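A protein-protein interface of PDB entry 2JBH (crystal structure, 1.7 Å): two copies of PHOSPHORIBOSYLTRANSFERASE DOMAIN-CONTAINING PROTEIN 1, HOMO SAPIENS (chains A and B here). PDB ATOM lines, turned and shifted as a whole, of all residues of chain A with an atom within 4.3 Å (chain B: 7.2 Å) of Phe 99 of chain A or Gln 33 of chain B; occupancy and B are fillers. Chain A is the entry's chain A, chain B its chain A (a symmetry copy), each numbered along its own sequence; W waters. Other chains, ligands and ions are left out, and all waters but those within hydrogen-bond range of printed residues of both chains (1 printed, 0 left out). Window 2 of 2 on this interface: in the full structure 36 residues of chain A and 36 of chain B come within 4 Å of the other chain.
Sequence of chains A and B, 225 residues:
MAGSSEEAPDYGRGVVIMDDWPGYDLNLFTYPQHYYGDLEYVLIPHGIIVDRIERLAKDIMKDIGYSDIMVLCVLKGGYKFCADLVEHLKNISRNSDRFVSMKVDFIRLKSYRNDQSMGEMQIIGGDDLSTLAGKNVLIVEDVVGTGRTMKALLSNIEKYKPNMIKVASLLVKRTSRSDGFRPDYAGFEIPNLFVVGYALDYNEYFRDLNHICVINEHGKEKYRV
The side-chain amide nitrogen of Gln 33 of chain B lies within hydrogen-bond range of the backbone carbonyl oxygen of Ser 96 of chain A (2.8 Å). The backbone carbonyl oxygen (O) of Ser 93 of chain A lies within hydrogen-bond range of the side-chain amide nitrogen (NE2) of Gln 33 of chain B (2.9 Å).
The side-chain hydroxyl (OG) of Ser 96 of chain A sits at hydrogen-bond distance from the backbone NH (N) of Arg 98 of chain A, 2.9 Å away. The backbone NH of Val 100 of chain A lies within hydrogen-bond range of the side-chain hydroxyl of Ser 93 of chain A (2.8 Å).
Among the printed residues, pairs that only touch across the chains: Val 100 of chain A with His 34 of chain B (3.0 Å), Arg 94 of chain A with Tyr 31 of chain B (3.2 Å), Phe 99 of chain A with Gln 33 of chain B (3.4 Å), Arg 94 of chain A with Thr 30 of chain B (3.4 Å), Arg 94 of chain A with Gln 33 of chain B (3.8 Å), Ser 93 of chain A with Pro 32 of chain B (3.9 Å) and Phe 99 of chain A with His 34 of chain B (3.9 Å).
Of the printed residues of chain A, Gln 33 of chain B touches Ser 93 (2.9 Å), Arg 94 (3.8 Å), Ser 96 (2.8 Å) and Phe 99 (3.4 Å). Of the printed residues of chain A, Pro 32 of chain B touches Ser 93 (3.9 Å). Of the printed residues of chain A, Tyr 31 of chain B touches Arg 94. The nearest printed residue of chain B that does not touch Arg 94 of chain A is Pro 32 of chain B (4.01 Å).
Of the 9 printed residues of chain A, 5 touch a printed residue of chain B. Hydrophobic or aromatic side chains of chain B within 4 Å of the printed part of chain A: His 34. Along chain B the printed residues that touch a printed residue of chain A span positions 30 to 34. Among the printed residues, no Asp or Glu carboxylate lies within 4 Å of a Lys or Arg side-chain nitrogen of the other chain.
No position is printed for both chains.
Water W1 bridges O of Arg 94 of chain A (2.7 Å) and O of Tyr 31 of chain B (2.9 Å).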
ATOM      1  N   MET A  61      26.509   3.693  22.030  1.00  0.00           N
ATOM      2  CA  MET A  61      25.565   4.729  22.465  1.00  0.00           C
ATOM      3  C   MET A  61      25.717   4.996  23.968  1.00  0.00           C
ATOM      4  O   MET A  61      25.704   6.156  24.402  1.00  0.00           O
ATOM      5  CB  MET A  61      24.144   4.316  22.135  1.00  0.00           C
ATOM      6  CG  MET A  61      23.608   4.952  20.880  1.00  0.00           C
ATOM      7  SD  MET A  61      23.284   6.742  21.057  1.00  0.00           S
ATOM      8  CE  MET A  61      21.940   6.861  19.885  1.00  0.00           C
ATOM      9  N   GLY A  65      27.365   8.288  23.265  1.00  0.00           N
ATOM     10  CA  GLY A  65      26.134   8.900  22.744  1.00  0.00           C
ATOM     11  C   GLY A  65      25.814  10.253  23.366  1.00  0.00           C
ATOM     12  O   GLY A  65      24.922  10.953  22.896  1.00  0.00           O
ATOM     13  N   SER A  93      18.706   6.292  17.581  1.00  0.00           N
ATOM     14  CA  SER A  93      18.474   7.734  17.619  1.00  0.00           C
ATOM     15  C   SER A  93      17.046   8.129  17.215  1.00  0.00           C
ATOM     16  O   SER A  93      16.557   9.234  17.547  1.00  0.00           O
ATOM     17  CB  SER A  93      19.509   8.442  16.754  1.00  0.00           C
ATOM     18  OG  SER A  93      20.745   8.519  17.438  1.00  0.00           O
ATOM     19  N   ARG A  94      16.360   7.243  16.501  1.00  0.00           N
ATOM     20  CA  ARG A  94      14.989   7.581  16.147  1.00  0.00           C
ATOM     21  C   ARG A  94      13.892   6.848  16.953  1.00  0.00           C
ATOM     22  O   ARG A  94      12.821   7.407  17.167  1.00  0.00           O
ATOM     23  CB  ARG A  94      14.756   7.569  14.643  1.00  0.00           C
ATOM     24  CG  ARG A  94      14.897   6.258  13.982  1.00  0.00           C
ATOM     25  CD  ARG A  94      14.594   6.392  12.505  1.00  0.00           C
ATOM     26  NE  ARG A  94      14.470   5.047  11.987  1.00  0.00           N
ATOM     27  CZ  ARG A  94      15.469   4.359  11.453  1.00  0.00           C
ATOM     28  NH1 ARG A  94      16.673   4.931  11.298  1.00  0.00           N
ATOM     29  NH2 ARG A  94      15.245   3.106  11.056  1.00  0.00           N
ATOM     30  N   SER A  96      14.281   5.081  20.149  1.00  0.00           N
ATOM     31  CA  SER A  96      14.417   5.083  21.594  1.00  0.00           C
ATOM     32  C   SER A  96      14.346   6.504  22.140  1.00  0.00           C
ATOM     33  O   SER A  96      13.910   7.437  21.449  1.00  0.00           O
ATOM     34  CB  SER A  96      15.720   4.408  22.020  1.00  0.00           C
ATOM     35  OG  SER A  96      16.791   5.339  22.051  1.00  0.00           O
ATOM     36  N   ASP A  97      14.788   6.635  23.388  1.00  0.00           N
ATOM     37  CA  ASP A  97      14.793   7.841  24.190  1.00  0.00           C
ATOM     38  C   ASP A  97      16.160   8.522  24.118  1.00  0.00           C
ATOM     39  O   ASP A  97      16.363   9.617  24.663  1.00  0.00           O
ATOM     40  CB  ASP A  97      14.499   7.427  25.644  1.00  0.00           C
ATOM     41  CG  ASP A  97      14.714   5.917  25.892  1.00  0.00           C
ATOM     42  OD1 ASP A  97      15.812   5.373  25.608  1.00  0.00           O
ATOM     43  OD2 ASP A  97      13.766   5.269  26.380  1.00  0.00           O
ATOM     44  N   ARG A  98      17.095   7.820  23.485  1.00  0.00           N
ATOM     45  CA  ARG A  98      18.495   8.190  23.440  1.00  0.00           C
ATOM     46  C   ARG A  98      18.869   8.562  22.011  1.00  0.00           C
ATOM     47  O   ARG A  98      18.696   7.762  21.108  1.00  0.00           O
ATOM     48  CB  ARG A  98      19.302   6.968  23.876  1.00  0.00           C
ATOM     49  CG  ARG A  98      20.581   7.267  24.583  1.00  0.00           C
ATOM     50  CD  ARG A  98      21.029   6.058  25.397  1.00  0.00           C
ATOM     51  NE  ARG A  98      20.415   5.986  26.725  1.00  0.00           N
ATOM     52  CZ  ARG A  98      20.797   6.722  27.772  1.00  0.00           C
ATOM     53  NH1 ARG A  98      21.784   7.602  27.652  1.00  0.00           N
ATOM     54  NH2 ARG A  98      20.185   6.583  28.944  1.00  0.00           N
ATOM     55  N   PHE A  99      19.363   9.770  21.783  1.00  0.00           N
ATOM     56  CA  PHE A  99      19.739  10.116  20.410  1.00  0.00           C
ATOM     57  C   PHE A  99      21.141  10.648  20.286  1.00  0.00           C
ATOM     58  O   PHE A  99      21.669  11.205  21.236  1.00  0.00           O
ATOM     59  CB  PHE A  99      18.723  11.051  19.746  1.00  0.00           C
ATOM     60  CG  PHE A  99      18.048  12.018  20.678  1.00  0.00           C
ATOM     61  CD1 PHE A  99      16.873  11.659  21.340  1.00  0.00           C
ATOM     62  CD2 PHE A  99      18.542  13.299  20.841  1.00  0.00           C
ATOM     63  CE1 PHE A  99      16.221  12.560  22.171  1.00  0.00           C
ATOM     64  CE2 PHE A  99      17.898  14.215  21.670  1.00  0.00           C
ATOM     65  CZ  PHE A  99      16.734  13.849  22.330  1.00  0.00           C
ATOM     66  N   VAL A 100      21.769  10.451  19.127  1.00  0.00           N
ATOM     67  CA  VAL A 100      23.089  11.046  18.898  1.00  0.00           C
ATOM     68  C   VAL A 100      23.194  11.580  17.475  1.00  0.00           C
ATOM     69  O   VAL A 100      22.784  10.902  16.534  1.00  0.00           O
ATOM     70  CB  VAL A 100      24.258  10.060  19.208  1.00  0.00           C
ATOM     71  CG1 VAL A 100      24.348   8.912  18.172  1.00  0.00           C
ATOM     72  CG2 VAL A 100      25.569  10.818  19.294  1.00  0.00           C
ATOM     73  N   THR B  30       9.127   8.277  12.075  1.00  0.00           N
ATOM     74  CA  THR B  30      10.236   8.465  13.017  1.00  0.00           C
ATOM     75  C   THR B  30      11.378   9.128  12.268  1.00  0.00           C
ATOM     76  O   THR B  30      11.457   9.024  11.035  1.00  0.00           O
ATOM     77  CB  THR B  30      10.765   7.166  13.640  1.00  0.00           C
ATOM     78  OG1 THR B  30      11.221   6.291  12.592  1.00  0.00           O
ATOM     79  CG2 THR B  30       9.677   6.488  14.477  1.00  0.00           C
ATOM     80  N   TYR B  31      12.241   9.807  13.017  1.00  0.00           N
ATOM     81  CA  TYR B  31      13.367  10.563  12.449  1.00  0.00           C
ATOM     82  C   TYR B  31      14.323  10.851  13.602  1.00  0.00           C
ATOM     83  O   TYR B  31      13.934  10.708  14.771  1.00  0.00           O
ATOM     84  CB  TYR B  31      12.862  11.870  11.810  1.00  0.00           C
ATOM     85  CG  TYR B  31      12.060  12.705  12.776  1.00  0.00           C
ATOM     86  CD1 TYR B  31      10.666  12.657  12.775  1.00  0.00           C
ATOM     87  CD2 TYR B  31      12.693  13.505  13.734  1.00  0.00           C
ATOM     88  CE1 TYR B  31       9.915  13.401  13.687  1.00  0.00           C
ATOM     89  CE2 TYR B  31      11.955  14.254  14.653  1.00  0.00           C
ATOM     90  CZ  TYR B  31      10.569  14.198  14.625  1.00  0.00           C
ATOM     91  OH  TYR B  31       9.842  14.933  15.542  1.00  0.00           O
ATOM     92  N   PRO B  32      15.568  11.261  13.301  1.00  0.00           N
ATOM     93  CA  PRO B  32      16.516  11.491  14.386  1.00  0.00           C
ATOM     94  C   PRO B  32      16.023  12.627  15.271  1.00  0.00           C
ATOM     95  O   PRO B  32      15.732  13.727  14.792  1.00  0.00           O
ATOM     96  CB  PRO B  32      17.814  11.875  13.659  1.00  0.00           C
ATOM     97  CG  PRO B  32      17.639  11.390  12.264  1.00  0.00           C
ATOM     98  CD  PRO B  32      16.165  11.534  11.983  1.00  0.00           C
ATOM     99  N   GLN B  33      15.921  12.361  16.567  1.00  0.00           N
ATOM    100  CA  GLN B  33      15.276  13.319  17.455  1.00  0.00           C
ATOM    101  C   GLN B  33      16.062  14.633  17.596  1.00  0.00           C
ATOM    102  O   GLN B  33      15.494  15.683  17.884  1.00  0.00           O
ATOM    103  CB  GLN B  33      14.927  12.645  18.793  1.00  0.00           C
ATOM    104  CG  GLN B  33      13.911  11.478  18.583  1.00  0.00           C
ATOM    105  CD  GLN B  33      13.821  10.465  19.735  1.00  0.00           C
ATOM    106  OE1 GLN B  33      12.925  10.560  20.607  1.00  0.00           O
ATOM    107  NE2 GLN B  33      14.716   9.476  19.729  1.00  0.00           N
ATOM    108  N   HIS B  34      17.367  14.588  17.335  1.00  0.00           N
ATOM    109  CA  HIS B  34      18.160  15.812  17.304  1.00  0.00           C
ATOM    110  C   HIS B  34      17.768  16.790  16.182  1.00  0.00           C
ATOM    111  O   HIS B  34      18.186  17.955  16.201  1.00  0.00           O
ATOM    112  CB  HIS B  34      19.667  15.512  17.269  1.00  0.00           C
ATOM    113  CG  HIS B  34      20.053  14.415  16.328  1.00  0.00           C
ATOM    114  ND1 HIS B  34      19.792  13.079  16.581  1.00  0.00           N
ATOM    115  CD2 HIS B  34      20.691  14.458  15.130  1.00  0.00           C
ATOM    116  CE1 HIS B  34      20.278  12.355  15.585  1.00  0.00           C
ATOM    117  NE2 HIS B  34      20.829  13.169  14.697  1.00  0.00           N
ATOM    118  N   TYR B  35      16.973  16.330  15.216  1.00  0.00           N
ATOM    119  CA  TYR B  35      16.461  17.216  14.153  1.00  0.00           C
ATOM    120  C   TYR B  35      15.011  17.662  14.359  1.00  0.00           C
ATOM    121  O   TYR B  35      14.397  18.259  13.459  1.00  0.00           O
ATOM    122  CB  TYR B  35      16.604  16.569  12.759  1.00  0.00           C
ATOM    123  CG  TYR B  35      18.033  16.204  12.407  1.00  0.00           C
ATOM    124  CD1 TYR B  35      19.084  17.117  12.601  1.00  0.00           C
ATOM    125  CD2 TYR B  35      18.335  14.957  11.868  1.00  0.00           C
ATOM    126  CE1 TYR B  35      20.417  16.780  12.290  1.00  0.00           C
ATOM    127  CE2 TYR B  35      19.651  14.589  11.557  1.00  0.00           C
ATOM    128  CZ  TYR B  35      20.702  15.508  11.768  1.00  0.00           C
ATOM    129  OH  TYR B  35      22.019  15.177  11.471  1.00  0.00           O
ATOM    130  N   TYR B  36      14.465  17.376  15.534  1.00  0.00           N
ATOM    131  CA  TYR B  36      13.131  17.854  15.859  1.00  0.00           C
ATOM    132  C   TYR B  36      13.111  19.382  15.711  1.00  0.00           C
ATOM    133  O   TYR B  36      13.960  20.070  16.269  1.00  0.00           O
ATOM    134  CB  TYR B  36      12.735  17.434  17.273  1.00  0.00           C
ATOM    135  CG  TYR B  36      11.401  18.006  17.721  1.00  0.00           C
ATOM    136  CD1 TYR B  36      10.200  17.416  17.324  1.00  0.00           C
ATOM    137  CD2 TYR B  36      11.343  19.146  18.527  1.00  0.00           C
ATOM    138  CE1 TYR B  36       8.962  17.939  17.728  1.00  0.00           C
ATOM    139  CE2 TYR B  36      10.113  19.684  18.932  1.00  0.00           C
ATOM    140  CZ  TYR B  36       8.934  19.072  18.533  1.00  0.00           C
ATOM    141  OH  TYR B  36       7.725  19.597  18.933  1.00  0.00           O
ATOM    142  N   GLY B  37      12.169  19.890  14.924  1.00  0.00           N
ATOM    143  CA  GLY B  37      12.021  21.344  14.744  1.00  0.00           C
ATOM    144  C   GLY B  37      12.858  21.929  13.609  1.00  0.00           C
ATOM    145  O   GLY B  37      12.797  23.132  13.335  1.00  0.00           O
ATOM    146  N   ASP B  38      13.652  21.077  12.950  1.00  0.00           N
ATOM    147  CA  ASP B  38      14.625  21.507  11.929  1.00  0.00           C
ATOM    148  C   ASP B  38      14.227  21.125  10.489  1.00  0.00           C
ATOM    149  O   ASP B  38      14.898  21.523   9.524  1.00  0.00           O
ATOM    150  CB  ASP B  38      15.990  20.872  12.229  1.00  0.00           C
ATOM    151  CG  ASP B  38      16.586  21.345  13.544  1.00  0.00           C
ATOM    152  OD1 ASP B  38      16.176  22.419  14.038  1.00  0.00           O
ATOM    153  OD2 ASP B  38      17.469  20.634  14.069  1.00  0.00           O
ATOM    154  N   LYS B 222      20.120  27.224  11.820  1.00  0.00           N
ATOM    155  CA  LYS B 222      20.762  26.481  12.906  1.00  0.00           C
ATOM    156  C   LYS B 222      22.071  25.821  12.479  1.00  0.00           C
ATOM    157  O   LYS B 222      23.052  25.797  13.246  1.00  0.00           O
ATOM    158  CB  LYS B 222      19.797  25.427  13.458  1.00  0.00           C
ATOM    159  CG  LYS B 222      20.330  24.601  14.626  1.00  0.00           C
ATOM    160  CD  LYS B 222      19.245  23.662  15.081  1.00  0.00           C
ATOM    161  CE  LYS B 222      19.730  22.699  16.156  1.00  0.00           C
ATOM    162  NZ  LYS B 222      18.578  21.853  16.577  1.00  0.00           N
HETATM  163  O   HOH W   1      11.580   9.590  16.056  1.00  0.00           O
